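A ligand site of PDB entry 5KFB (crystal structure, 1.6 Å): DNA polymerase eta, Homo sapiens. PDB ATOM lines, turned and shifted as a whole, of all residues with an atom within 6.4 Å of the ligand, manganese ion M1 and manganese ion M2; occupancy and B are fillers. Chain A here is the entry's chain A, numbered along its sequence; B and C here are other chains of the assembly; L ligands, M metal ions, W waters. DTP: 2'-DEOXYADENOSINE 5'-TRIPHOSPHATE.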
ATOM      1  N   ASP A  16     -22.959  27.472  -4.135  1.00  0.00           N
ATOM      2  CA  ASP A  16     -22.314  26.960  -5.341  1.00  0.00           C
ATOM      3  C   ASP A  16     -22.592  25.479  -5.500  1.00  0.00           C
ATOM      4  O   ASP A  16     -22.337  24.683  -4.601  1.00  0.00           O
ATOM      5  CB  ASP A  16     -20.807  27.189  -5.292  1.00  0.00           C
ATOM      6  CG  ASP A  16     -20.116  26.664  -6.530  1.00  0.00           C
ATOM      7  OD1 ASP A  16     -19.766  25.470  -6.530  1.00  0.00           O
ATOM      8  OD2 ASP A  16     -19.947  27.442  -7.497  1.00  0.00           O
ATOM      9  N   MET A  17     -23.109  25.096  -6.668  1.00  0.00           N
ATOM     10  CA  MET A  17     -23.500  23.707  -6.866  1.00  0.00           C
ATOM     11  C   MET A  17     -22.311  22.757  -6.884  1.00  0.00           C
ATOM     12  O   MET A  17     -21.269  23.109  -7.404  1.00  0.00           O
ATOM     13  CB  MET A  17     -24.312  23.561  -8.159  1.00  0.00           C
ATOM     14  CG  MET A  17     -25.477  24.520  -8.252  1.00  0.00           C
ATOM     15  SD  MET A  17     -26.643  24.429  -6.865  1.00  0.00           S
ATOM     16  CE  MET A  17     -27.193  22.764  -6.991  1.00  0.00           C
ATOM     17  N   ASP A  18     -22.469  21.573  -6.302  1.00  0.00           N
ATOM     18  CA  ASP A  18     -21.380  20.591  -6.349  1.00  0.00           C
ATOM     19  C   ASP A  18     -21.313  19.917  -7.709  1.00  0.00           C
ATOM     20  O   ASP A  18     -22.341  19.442  -8.215  1.00  0.00           O
ATOM     21  CB  ASP A  18     -21.564  19.490  -5.311  1.00  0.00           C
ATOM     22  CG  ASP A  18     -21.577  20.021  -3.873  1.00  0.00           C
ATOM     23  OD1 ASP A  18     -20.947  21.064  -3.597  1.00  0.00           O
ATOM     24  OD2 ASP A  18     -22.208  19.355  -3.037  1.00  0.00           O
ATOM     25  N   CYS A  19     -20.113  19.896  -8.283  1.00  0.00           N
ATOM     26  CA  CYS A  19     -19.808  19.299  -9.599  1.00  0.00           C
ATOM     27  C   CYS A  19     -21.026  19.374 -10.526  1.00  0.00           C
ATOM     28  O   CYS A  19     -21.586  18.360 -10.932  1.00  0.00           O
ATOM     29  CB  CYS A  19     -19.309  17.833  -9.468  1.00  0.00           C
ATOM     30  SG  CYS A  19     -20.296  16.656  -8.524  1.00  0.00           S
ATOM     31  N   PHE A  20     -21.427  20.610 -10.825  1.00  0.00           N
ATOM     32  CA  PHE A  20     -22.782  20.887 -11.292  1.00  0.00           C
ATOM     33  C   PHE A  20     -23.203  20.098 -12.539  1.00  0.00           C
ATOM     34  O   PHE A  20     -24.221  19.417 -12.498  1.00  0.00           O
ATOM     35  CB  PHE A  20     -22.971  22.389 -11.555  1.00  0.00           C
ATOM     36  CG  PHE A  20     -24.381  22.775 -11.931  1.00  0.00           C
ATOM     37  CD1 PHE A  20     -25.462  22.282 -11.225  1.00  0.00           C
ATOM     38  CD2 PHE A  20     -24.622  23.618 -13.012  1.00  0.00           C
ATOM     39  CE1 PHE A  20     -26.776  22.647 -11.568  1.00  0.00           C
ATOM     40  CE2 PHE A  20     -25.933  23.986 -13.365  1.00  0.00           C
ATOM     41  CZ  PHE A  20     -27.000  23.499 -12.639  1.00  0.00           C
ATOM     42  N   PHE A  21     -22.436  20.185 -13.628  1.00  0.00           N
ATOM     43  CA  PHE A  21     -22.900  19.523 -14.853  1.00  0.00           C
ATOM     44  C   PHE A  21     -22.983  18.014 -14.636  1.00  0.00           C
ATOM     45  O   PHE A  21     -23.829  17.350 -15.229  1.00  0.00           O
ATOM     46  CB  PHE A  21     -21.992  19.808 -16.069  1.00  0.00           C
ATOM     47  CG  PHE A  21     -22.049  21.214 -16.601  1.00  0.00           C
ATOM     48  CD1 PHE A  21     -22.689  22.244 -15.904  1.00  0.00           C
ATOM     49  CD2 PHE A  21     -21.479  21.498 -17.821  1.00  0.00           C
ATOM     50  CE1 PHE A  21     -22.718  23.540 -16.449  1.00  0.00           C
ATOM     51  CE2 PHE A  21     -21.519  22.780 -18.374  1.00  0.00           C
ATOM     52  CZ  PHE A  21     -22.130  23.797 -17.669  1.00  0.00           C
ATOM     53  N   VAL A  22     -22.110  17.470 -13.798  1.00  0.00           N
ATOM     54  CA  VAL A  22     -22.164  16.046 -13.486  1.00  0.00           C
ATOM     55  C   VAL A  22     -23.479  15.714 -12.767  1.00  0.00           C
ATOM     56  O   VAL A  22     -24.158  14.740 -13.120  1.00  0.00           O
ATOM     57  CB  VAL A  22     -20.958  15.605 -12.647  1.00  0.00           C
ATOM     58  CG1 VAL A  22     -21.208  14.248 -11.966  1.00  0.00           C
ATOM     59  CG2 VAL A  22     -19.688  15.552 -13.519  1.00  0.00           C
ATOM     60  N   GLN A  41     -16.950  17.398 -23.606  1.00  0.00           N
ATOM     61  CA  GLN A  41     -17.490  17.959 -24.843  1.00  0.00           C
ATOM     62  C   GLN A  41     -16.606  17.558 -25.994  1.00  0.00           C
ATOM     63  O   GLN A  41     -15.373  17.572 -25.901  1.00  0.00           O
ATOM     64  CB  GLN A  41     -17.688  19.479 -24.766  1.00  0.00           C
ATOM     65  CG  GLN A  41     -16.498  20.278 -24.349  1.00  0.00           C
ATOM     66  CD  GLN A  41     -16.871  21.726 -24.018  1.00  0.00           C
ATOM     67  OE1 GLN A  41     -18.050  22.101 -23.998  1.00  0.00           O
ATOM     68  NE2 GLN A  41     -15.865  22.537 -23.786  1.00  0.00           N
ATOM     69  N   ILE A  51     -15.109  18.850 -18.724  1.00  0.00           N
ATOM     70  CA  ILE A  51     -15.477  20.143 -18.147  1.00  0.00           C
ATOM     71  C   ILE A  51     -16.090  20.045 -16.751  1.00  0.00           C
ATOM     72  O   ILE A  51     -16.243  21.074 -16.090  1.00  0.00           O
ATOM     73  CB  ILE A  51     -16.433  20.940 -19.051  1.00  0.00           C
ATOM     74  CG1 ILE A  51     -17.742  20.180 -19.324  1.00  0.00           C
ATOM     75  CG2 ILE A  51     -15.729  21.322 -20.365  1.00  0.00           C
ATOM     76  CD1 ILE A  51     -18.777  21.017 -20.089  1.00  0.00           C
ATOM     77  N   ALA A  52     -16.413  18.845 -16.286  1.00  0.00           N
ATOM     78  CA  ALA A  52     -16.914  18.656 -14.918  1.00  0.00           C
ATOM     79  C   ALA A  52     -16.600  17.235 -14.442  1.00  0.00           C
ATOM     80  O   ALA A  52     -16.630  16.304 -15.248  1.00  0.00           O
ATOM     81  CB  ALA A  52     -18.419  18.932 -14.826  1.00  0.00           C
ATOM     82  N   VAL A  53     -16.314  17.072 -13.148  1.00  0.00           N
ATOM     83  CA  VAL A  53     -15.805  15.827 -12.582  1.00  0.00           C
ATOM     84  C   VAL A  53     -16.454  15.516 -11.246  1.00  0.00           C
ATOM     85  O   VAL A  53     -16.448  16.357 -10.332  1.00  0.00           O
ATOM     86  CB  VAL A  53     -14.270  15.900 -12.357  1.00  0.00           C
ATOM     87  CG1 VAL A  53     -13.723  14.545 -11.946  1.00  0.00           C
ATOM     88  CG2 VAL A  53     -13.554  16.388 -13.610  1.00  0.00           C
ATOM     89  N   TYR A  55     -16.913  13.822  -7.512  1.00  0.00           N
ATOM     90  CA  TYR A  55     -15.927  13.728  -6.439  1.00  0.00           C
ATOM     91  C   TYR A  55     -15.289  12.345  -6.359  1.00  0.00           C
ATOM     92  O   TYR A  55     -14.118  12.230  -6.029  1.00  0.00           O
ATOM     93  CB  TYR A  55     -16.559  14.136  -5.103  1.00  0.00           C
ATOM     94  CG  TYR A  55     -16.622  15.649  -5.017  1.00  0.00           C
ATOM     95  CD1 TYR A  55     -17.639  16.355  -5.660  1.00  0.00           C
ATOM     96  CD2 TYR A  55     -15.617  16.373  -4.374  1.00  0.00           C
ATOM     97  CE1 TYR A  55     -17.664  17.740  -5.656  1.00  0.00           C
ATOM     98  CE2 TYR A  55     -15.652  17.765  -4.350  1.00  0.00           C
ATOM     99  CZ  TYR A  55     -16.672  18.439  -4.981  1.00  0.00           C
ATOM    100  OH  TYR A  55     -16.693  19.814  -4.968  1.00  0.00           O
ATOM    101  N   ARG A  58     -12.557  12.569  -8.886  1.00  0.00           N
ATOM    102  CA  ARG A  58     -11.445  13.432  -8.459  1.00  0.00           C
ATOM    103  C   ARG A  58     -10.449  12.661  -7.598  1.00  0.00           C
ATOM    104  O   ARG A  58      -9.251  12.980  -7.602  1.00  0.00           O
ATOM    105  CB  ARG A  58     -11.970  14.633  -7.683  1.00  0.00           C
ATOM    106  CG  ARG A  58     -12.832  15.526  -8.518  1.00  0.00           C
ATOM    107  CD  ARG A  58     -13.315  16.732  -7.733  1.00  0.00           C
ATOM    108  NE  ARG A  58     -14.426  17.355  -8.464  1.00  0.00           N
ATOM    109  CZ  ARG A  58     -14.943  18.551  -8.204  1.00  0.00           C
ATOM    110  NH1 ARG A  58     -14.451  19.312  -7.240  1.00  0.00           N
ATOM    111  NH2 ARG A  58     -15.969  18.988  -8.958  1.00  0.00           N
ATOM    112  N   ARG A  64     -10.815  18.900 -14.525  1.00  0.00           N
ATOM    113  CA  ARG A  64     -11.222  19.728 -15.633  1.00  0.00           C
ATOM    114  C   ARG A  64     -10.029  19.981 -16.574  1.00  0.00           C
ATOM    115  O   ARG A  64      -8.876  19.995 -16.119  1.00  0.00           O
ATOM    116  CB  ARG A  64     -11.815  21.037 -15.109  1.00  0.00           C
ATOM    117  CG  ARG A  64     -12.172  22.083 -16.138  1.00  0.00           C
ATOM    118  CD  ARG A  64     -12.930  23.233 -15.474  1.00  0.00           C
ATOM    119  NE  ARG A  64     -14.203  22.736 -14.983  1.00  0.00           N
ATOM    120  CZ  ARG A  64     -14.714  22.952 -13.771  1.00  0.00           C
ATOM    121  NH1 ARG A  64     -14.076  23.704 -12.874  1.00  0.00           N
ATOM    122  NH2 ARG A  64     -15.875  22.416 -13.460  1.00  0.00           N
ATOM    123  N   LEU A  92     -25.174  24.191 -24.506  1.00  0.00           N
ATOM    124  CA  LEU A  92     -25.230  24.087 -23.041  1.00  0.00           C
ATOM    125  C   LEU A  92     -26.630  24.311 -22.450  1.00  0.00           C
ATOM    126  O   LEU A  92     -26.762  24.542 -21.258  1.00  0.00           O
ATOM    127  CB  LEU A  92     -24.265  25.080 -22.406  1.00  0.00           C
ATOM    128  CG  LEU A  92     -22.832  25.002 -22.937  1.00  0.00           C
ATOM    129  CD1 LEU A  92     -21.973  26.112 -22.343  1.00  0.00           C
ATOM    130  CD2 LEU A  92     -22.257  23.641 -22.572  1.00  0.00           C
ATOM    131  N   SER A 116     -22.456  32.940 -11.707  1.00  0.00           N
ATOM    132  CA  SER A 116     -22.054  32.003 -12.743  1.00  0.00           C
ATOM    133  C   SER A 116     -23.231  31.082 -13.045  1.00  0.00           C
ATOM    134  O   SER A 116     -24.299  31.203 -12.453  1.00  0.00           O
ATOM    135  CB  SER A 116     -20.858  31.161 -12.295  1.00  0.00           C
ATOM    136  OG  SER A 116     -21.297  30.091 -11.476  1.00  0.00           O
ATOM    137  N   ILE A 117     -23.033  30.127 -13.946  1.00  0.00           N
ATOM    138  CA  ILE A 117     -24.088  29.194 -14.259  1.00  0.00           C
ATOM    139  C   ILE A 117     -24.492  28.353 -13.025  1.00  0.00           C
ATOM    140  O   ILE A 117     -25.595  27.828 -12.958  1.00  0.00           O
ATOM    141  CB  ILE A 117     -23.690  28.260 -15.431  1.00  0.00           C
ATOM    142  CG1 ILE A 117     -24.939  27.648 -16.082  1.00  0.00           C
ATOM    143  CG2 ILE A 117     -22.687  27.201 -14.963  1.00  0.00           C
ATOM    144  CD1 ILE A 117     -24.651  26.932 -17.409  1.00  0.00           C
ATOM    145  N   ASP A 118     -23.595  28.228 -12.044  1.00  0.00           N
ATOM    146  CA  ASP A 118     -23.947  27.351 -10.924  1.00  0.00           C
ATOM    147  C   ASP A 118     -23.772  28.006  -9.550  1.00  0.00           C
ATOM    148  O   ASP A 118     -23.690  27.305  -8.534  1.00  0.00           O
ATOM    149  CB  ASP A 118     -23.131  26.048 -10.983  1.00  0.00           C
ATOM    150  CG  ASP A 118     -21.787  26.148 -10.287  1.00  0.00           C
ATOM    151  OD1 ASP A 118     -21.092  27.204 -10.375  1.00  0.00           O
ATOM    152  OD2 ASP A 118     -21.432  25.168  -9.586  1.00  0.00           O
ATOM    153  N   GLU A 119     -23.724  29.330  -9.491  1.00  0.00           N
ATOM    154  CA  GLU A 119     -23.612  29.944  -8.178  1.00  0.00           C
ATOM    155  C   GLU A 119     -24.186  31.338  -8.104  1.00  0.00           C
ATOM    156  O   GLU A 119     -24.291  32.045  -9.104  1.00  0.00           O
ATOM    157  CB  GLU A 119     -22.151  29.984  -7.724  1.00  0.00           C
ATOM    158  CG  GLU A 119     -21.316  31.065  -8.355  1.00  0.00           C
ATOM    159  CD  GLU A 119     -19.861  30.673  -8.402  1.00  0.00           C
ATOM    160  OE1 GLU A 119     -19.071  31.168  -7.582  1.00  0.00           O
ATOM    161  OE2 GLU A 119     -19.503  29.840  -9.265  1.00  0.00           O
ATOM    162  N   SER A 216     -22.748  23.421  -1.961  1.00  0.00           N
ATOM    163  CA  SER A 216     -22.034  23.931  -0.807  1.00  0.00           C
ATOM    164  C   SER A 216     -22.302  25.409  -0.670  1.00  0.00           C
ATOM    165  O   SER A 216     -22.853  26.031  -1.588  1.00  0.00           O
ATOM    166  CB  SER A 216     -20.543  23.659  -0.958  1.00  0.00           C
ATOM    167  OG  SER A 216     -20.327  22.252  -1.059  1.00  0.00           O
ATOM    168  N   LYS A 227     -17.394  33.562  -0.698  1.00  0.00           N
ATOM    169  CA  LYS A 227     -16.858  32.706  -1.754  1.00  0.00           C
ATOM    170  C   LYS A 227     -15.735  31.820  -1.238  1.00  0.00           C
ATOM    171  O   LYS A 227     -15.701  30.609  -1.487  1.00  0.00           O
ATOM    172  CB  LYS A 227     -16.362  33.558  -2.936  1.00  0.00           C
ATOM    173  CG  LYS A 227     -15.723  32.721  -4.056  1.00  0.00           C
ATOM    174  CD  LYS A 227     -16.689  31.688  -4.647  1.00  0.00           C
ATOM    175  CE  LYS A 227     -16.021  30.885  -5.767  1.00  0.00           C
ATOM    176  NZ  LYS A 227     -16.919  29.889  -6.431  1.00  0.00           N
ATOM    177  N   LYS A 234     -16.089  21.183   0.856  1.00  0.00           N
ATOM    178  CA  LYS A 234     -17.070  20.944  -0.243  1.00  0.00           C
ATOM    179  C   LYS A 234     -16.754  19.449  -0.275  1.00  0.00           C
ATOM    180  O   LYS A 234     -15.661  19.097   0.061  1.00  0.00           O
ATOM    181  CB  LYS A 234     -16.859  21.590  -1.606  1.00  0.00           C
ATOM    182  CG  LYS A 234     -15.452  21.810  -1.985  1.00  0.00           C
ATOM    183  CD  LYS A 234     -15.331  22.543  -3.313  1.00  0.00           C
ATOM    184  CE  LYS A 234     -14.271  21.852  -4.181  1.00  0.00           C
ATOM    185  NZ  LYS A 234     -13.969  22.632  -5.419  1.00  0.00           N
ATOM    186  N   PRO A 235     -17.653  18.586  -0.727  1.00  0.00           N
ATOM    187  CA  PRO A 235     -18.993  18.944  -1.208  1.00  0.00           C
ATOM    188  C   PRO A 235     -20.060  18.836  -0.136  1.00  0.00           C
ATOM    189  O   PRO A 235     -19.797  18.288   0.936  1.00  0.00           O
ATOM    190  CB  PRO A 235     -19.252  17.906  -2.288  1.00  0.00           C
ATOM    191  CG  PRO A 235     -18.598  16.664  -1.717  1.00  0.00           C
ATOM    192  CD  PRO A 235     -17.372  17.155  -0.956  1.00  0.00           C
ATOM    193  P    DT B   8     -13.635  30.852 -10.356  1.00  0.00           P
ATOM    194  OP1  DT B   8     -14.019  30.542  -8.955  1.00  0.00           O
ATOM    195  OP2  DT B   8     -12.516  30.100 -10.993  1.00  0.00           O
ATOM    196  O5'  DT B   8     -14.911  30.644 -11.317  1.00  0.00           O
ATOM    197  C5'  DT B   8     -16.270  31.033 -10.973  1.00  0.00           C
ATOM    198  C4'  DT B   8     -17.196  30.285 -11.918  1.00  0.00           C
ATOM    199  O4'  DT B   8     -16.668  30.563 -13.236  1.00  0.00           O
ATOM    200  C3'  DT B   8     -17.054  28.787 -11.673  1.00  0.00           C
ATOM    201  O3'  DT B   8     -18.331  28.202 -11.550  1.00  0.00           O
ATOM    202  C2'  DT B   8     -16.300  28.274 -12.914  1.00  0.00           C
ATOM    203  C1'  DT B   8     -16.580  29.350 -13.948  1.00  0.00           C
ATOM    204  N1   DT B   8     -15.505  29.479 -14.953  1.00  0.00           N
ATOM    205  C2   DT B   8     -15.813  29.291 -16.278  1.00  0.00           C
ATOM    206  O2   DT B   8     -16.925  29.023 -16.661  1.00  0.00           O
ATOM    207  N3   DT B   8     -14.746  29.421 -17.140  1.00  0.00           N
ATOM    208  C4   DT B   8     -13.442  29.722 -16.813  1.00  0.00           C
ATOM    209  O4   DT B   8     -12.566  29.829 -17.659  1.00  0.00           O
ATOM    210  C5   DT B   8     -13.186  29.895 -15.402  1.00  0.00           C
ATOM    211  C7   DT B   8     -11.803  30.241 -14.927  1.00  0.00           C
ATOM    212  C6   DT B   8     -14.216  29.775 -14.555  1.00  0.00           C
ATOM    213  P    DT C   3      -4.252  22.106 -25.788  1.00  0.00           P
ATOM    214  OP1  DT C   3      -3.448  23.286 -26.185  1.00  0.00           O
ATOM    215  OP2  DT C   3      -3.609  20.913 -25.217  1.00  0.00           O
ATOM    216  O5'  DT C   3      -5.400  22.601 -24.793  1.00  0.00           O
ATOM    217  C5'  DT C   3      -6.504  21.764 -24.510  1.00  0.00           C
ATOM    218  C4'  DT C   3      -7.589  22.540 -23.794  1.00  0.00           C
ATOM    219  O4'  DT C   3      -7.244  22.674 -22.404  1.00  0.00           O
ATOM    220  C3'  DT C   3      -7.814  23.962 -24.334  1.00  0.00           C
ATOM    221  O3'  DT C   3      -9.147  24.106 -24.812  1.00  0.00           O
ATOM    222  C2'  DT C   3      -7.515  24.880 -23.130  1.00  0.00           C
ATOM    223  C1'  DT C   3      -7.671  23.935 -21.951  1.00  0.00           C
ATOM    224  N1   DT C   3      -6.822  24.311 -20.784  1.00  0.00           N
ATOM    225  C2   DT C   3      -7.433  24.593 -19.581  1.00  0.00           C
ATOM    226  O2   DT C   3      -8.644  24.542 -19.418  1.00  0.00           O
ATOM    227  N3   DT C   3      -6.574  24.921 -18.572  1.00  0.00           N
ATOM    228  C4   DT C   3      -5.192  24.992 -18.636  1.00  0.00           C
ATOM    229  O4   DT C   3      -4.503  25.309 -17.678  1.00  0.00           O
ATOM    230  C5   DT C   3      -4.624  24.688 -19.931  1.00  0.00           C
ATOM    231  C7   DT C   3      -3.136  24.738 -20.128  1.00  0.00           C
ATOM    232  C6   DT C   3      -5.457  24.362 -20.930  1.00  0.00           C
ATOM    233  P    DT C   4      -9.398  24.456 -26.359  1.00  0.00           P
ATOM    234  OP1  DT C   4      -8.807  23.363 -27.164  1.00  0.00           O
ATOM    235  OP2  DT C   4      -8.953  25.854 -26.553  1.00  0.00           O
ATOM    236  O5'  DT C   4     -10.986  24.455 -26.526  1.00  0.00           O
ATOM    237  C5'  DT C   4     -11.718  23.252 -26.827  1.00  0.00           C
ATOM    238  C4'  DT C   4     -13.200  23.470 -26.509  1.00  0.00           C
ATOM    239  O4'  DT C   4     -13.306  23.725 -25.096  1.00  0.00           O
ATOM    240  C3'  DT C   4     -13.820  24.683 -27.209  1.00  0.00           C
ATOM    241  O3'  DT C   4     -15.167  24.400 -27.492  1.00  0.00           O
ATOM    242  C2'  DT C   4     -13.671  25.789 -26.153  1.00  0.00           C
ATOM    243  C1'  DT C   4     -13.907  24.984 -24.884  1.00  0.00           C
ATOM    244  N1   DT C   4     -13.335  25.528 -23.641  1.00  0.00           N
ATOM    245  C2   DT C   4     -14.043  25.363 -22.497  1.00  0.00           C
ATOM    246  O2   DT C   4     -15.151  24.871 -22.477  1.00  0.00           O
ATOM    247  N3   DT C   4     -13.446  25.837 -21.369  1.00  0.00           N
ATOM    248  C4   DT C   4     -12.211  26.414 -21.252  1.00  0.00           C
ATOM    249  O4   DT C   4     -11.768  26.800 -20.181  1.00  0.00           O
ATOM    250  C5   DT C   4     -11.471  26.536 -22.499  1.00  0.00           C
ATOM    251  C7   DT C   4     -10.110  27.162 -22.519  1.00  0.00           C
ATOM    252  C6   DT C   4     -12.064  26.083 -23.619  1.00  0.00           C
ATOM    253  P    DA C   5     -16.106  25.471 -28.233  1.00  0.00           P
ATOM    254  OP1  DA C   5     -16.962  24.701 -29.157  1.00  0.00           O
ATOM    255  OP2  DA C   5     -15.269  26.596 -28.714  1.00  0.00           O
ATOM    256  O5'  DA C   5     -16.996  26.061 -27.046  1.00  0.00           O
ATOM    257  C5'  DA C   5     -17.939  25.235 -26.389  1.00  0.00           C
ATOM    258  C4'  DA C   5     -18.731  26.053 -25.394  1.00  0.00           C
ATOM    259  O4'  DA C   5     -17.899  26.403 -24.253  1.00  0.00           O
ATOM    260  C3'  DA C   5     -19.272  27.376 -25.937  1.00  0.00           C
ATOM    261  O3'  DA C   5     -20.551  27.600 -25.376  1.00  0.00           O
ATOM    262  C2'  DA C   5     -18.257  28.392 -25.422  1.00  0.00           C
ATOM    263  C1'  DA C   5     -17.946  27.799 -24.041  1.00  0.00           C
ATOM    264  N9   DA C   5     -16.684  28.232 -23.498  1.00  0.00           N
ATOM    265  C8   DA C   5     -15.521  28.496 -24.177  1.00  0.00           C
ATOM    266  N7   DA C   5     -14.534  28.859 -23.397  1.00  0.00           N
ATOM    267  C5   DA C   5     -15.078  28.809 -22.115  1.00  0.00           C
ATOM    268  C6   DA C   5     -14.536  29.083 -20.847  1.00  0.00           C
ATOM    269  N6   DA C   5     -13.279  29.464 -20.638  1.00  0.00           N
ATOM    270  N1   DA C   5     -15.351  28.948 -19.781  1.00  0.00           N
ATOM    271  C2   DA C   5     -16.620  28.554 -19.977  1.00  0.00           C
ATOM    272  N3   DA C   5     -17.239  28.273 -21.121  1.00  0.00           N
ATOM    273  C4   DA C   5     -16.387  28.424 -22.166  1.00  0.00           C
HETATM  274  PG  DTP L   1     -17.248  22.075  -7.686  1.00  0.00           P
HETATM  275  O1G DTP L   1     -17.819  23.471  -7.621  1.00  0.00           O
HETATM  276  O2G DTP L   1     -17.996  21.094  -6.829  1.00  0.00           O
HETATM  277  O3G DTP L   1     -15.756  22.049  -7.364  1.00  0.00           O
HETATM  278  PB  DTP L   1     -18.076  22.299 -10.411  1.00  0.00           P
HETATM  279  O1B DTP L   1     -19.472  22.746 -10.029  1.00  0.00           O
HETATM  280  O2B DTP L   1     -18.098  21.374 -11.594  1.00  0.00           O
HETATM  281  O3B DTP L   1     -17.361  21.537  -9.189  1.00  0.00           O
HETATM  282  PA  DTP L   1     -17.453  25.056 -10.977  1.00  0.00           P
HETATM  283  O1A DTP L   1     -18.289  25.649  -9.879  1.00  0.00           O
HETATM  284  O2A DTP L   1     -16.088  25.713 -11.120  1.00  0.00           O
HETATM  285  O3A DTP L   1     -17.120  23.517 -10.757  1.00  0.00           O
HETATM  286  O5' DTP L   1     -18.177  25.173 -12.374  1.00  0.00           O
HETATM  287  C5' DTP L   1     -19.554  24.913 -12.504  1.00  0.00           C
HETATM  288  C4' DTP L   1     -19.835  24.305 -13.873  1.00  0.00           C
HETATM  289  O4' DTP L   1     -19.453  25.244 -14.859  1.00  0.00           O
HETATM  290  C3' DTP L   1     -19.067  23.100 -14.123  1.00  0.00           C
HETATM  291  O3' DTP L   1     -19.781  21.925 -13.686  1.00  0.00           O
HETATM  292  C2' DTP L   1     -18.883  23.076 -15.576  1.00  0.00           C
HETATM  293  C1' DTP L   1     -18.826  24.527 -15.935  1.00  0.00           C
HETATM  294  N9  DTP L   1     -17.492  24.990 -16.063  1.00  0.00           N
HETATM  295  C8  DTP L   1     -16.647  25.405 -15.088  1.00  0.00           C
HETATM  296  N7  DTP L   1     -15.475  25.760 -15.587  1.00  0.00           N
HETATM  297  C5  DTP L   1     -15.526  25.598 -16.922  1.00  0.00           C
HETATM  298  C6  DTP L   1     -14.638  25.794 -17.971  1.00  0.00           C
HETATM  299  N6  DTP L   1     -13.321  26.293 -17.689  1.00  0.00           N
HETATM  300  N1  DTP L   1     -15.003  25.502 -19.217  1.00  0.00           N
HETATM  301  C2  DTP L   1     -16.239  25.035 -19.513  1.00  0.00           C
HETATM  302  N3  DTP L   1     -17.144  24.841 -18.514  1.00  0.00           N
HETATM  303  C4  DTP L   1     -16.796  25.101 -17.241  1.00  0.00           C
HETATM  304 MN    MN M   1     -19.166  27.704  -9.380  1.00  0.00          MN
HETATM  305 MN    MN M   2     -19.776  24.370  -8.407  1.00  0.00          MN
HETATM  306  O   HOH W   1     -17.192  27.896  -8.476  1.00  0.00           O
HETATM  307  O   HOH W   2     -16.137  19.494 -11.773  1.00  0.00           O
HETATM  308  O   HOH W   3     -16.335  25.601  -7.020  1.00  0.00           O
HETATM  309  O   HOH W   4     -19.576  24.969 -19.911  1.00  0.00           O
HETATM  310  O   HOH W   5     -13.824  22.394  -9.099  1.00  0.00           O
HETATM  311  O   HOH W   6     -12.924  26.483 -14.592  1.00  0.00           O
HETATM  312  O   HOH W   7     -19.264  27.829 -17.033  1.00  0.00           O
HETATM  313  O   HOH W   8     -19.560  27.938 -13.749  1.00  0.00           O
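Water W6 bridges a nitrogen (N7) of the ligand (2.8 Å) and the guanidinium group of Arg 64 (3.5 Å). Water W7 lies within hydrogen-bond range of O2 of DT 8 of chain B and O4' of the ligand.
Three residues have an atom within 4 Å of manganese ion M2: Asp 16, Met 17 and Asp 118.
Residues that only touch manganese ion M1: Ser 116. Within 4 Å of manganese ion M1: Asp 16, Ser 116, Asp 118, Glu 119 and DT 8 of chain B.
The side-chain carboxylate (OD1) of Asp 18 sits at hydrogen-bond distance from the side-chain hydroxyl (OG) of Ser 216 (2.9 Å). N of Glu 119 lies within hydrogen-bond range of OG of Ser 116, 3.2 Å away. OG of Ser 116 lies within hydrogen-bond range of N of Asp 118 (3.0 Å). NE2 of Gln 41 sits at hydrogen-bond distance from O2 of DT 4 of chain C, 2.8 Å away. The side-chain amino group (NZ) of Lys 227 is in salt-bridge range of OP1 of DT 8 of chain B (3.9 Å). The backbone carbonyl oxygen (O) of Ser 216 sits at hydrogen-bond distance from the backbone NH (N) of Asp 16 (2.9 Å). OE1 of Glu 119 is in salt-bridge range of NZ of Lys 227, at 2.8 Å. NH1 of Arg 58 is in hydrogen-bond range of OH of Tyr 55, at 3.2 Å.
Manganese ion M2 is bound by OD1 of Asp 16 (2.2 Å), OD2 of Asp 118 (2.2 Å), O of Met 17 (2.2 Å), O1G of the ligand (2.3 Å), O1B of the ligand (2.3 Å) and O1A of the ligand (2.5 Å). Manganese ion M2 has six donor atoms within binding distance.
O2B of the ligand lies within salt-bridge range of NH2 of Arg 64, at 3.1 Å. N3 of DT 8 of chain B sits at hydrogen-bond distance from N6 of the ligand (3.5 Å). An oxygen (O2G) of the ligand sits at hydrogen-bond distance from the backbone NH (N) of Cys 19 (2.8 Å). The guanidinium group (NH1) of Arg 58 is in salt-bridge range of an oxygen (O3G) of the ligand (3.0 Å). The side-chain hydroxyl (OH) of Tyr 55 lies within hydrogen-bond range of an oxygen (O2G) of the ligand (2.6 Å). N of Phe 20 sits close to O1B of the ligand (3.0 Å). The side-chain amino group (NZ) of Lys 234 is in salt-bridge range of an oxygen (O3G) of the ligand (2.7 Å). The backbone NH (N) of Phe 21 sits at hydrogen-bond distance from an oxygen (O3') of the ligand, at 3.2 Å. O4 of DT 4 of chain C sits at hydrogen-bond distance from a nitrogen (N6) of the ligand, 3.0 Å away.
Manganese ion M1 is bound by OD2 of Asp 16, OE2 of Glu 119, water W1, OD1 of Asp 118, O1A of the ligand and O3' of DT 8 of chain B.
Merely in contact with the ligand: Asp 18 (3.5 Å), Ile 51 (3.4 Å), Ala 52 (3.5 Å), Ile 117 (3.8 Å) and DA 5 of chain C (3.5 Å). Of the 27 residues printed, 17 come within 4 Å of the ligand. The nearest printed residue that does not touch the ligand is Glu 119 (4.4 Å).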
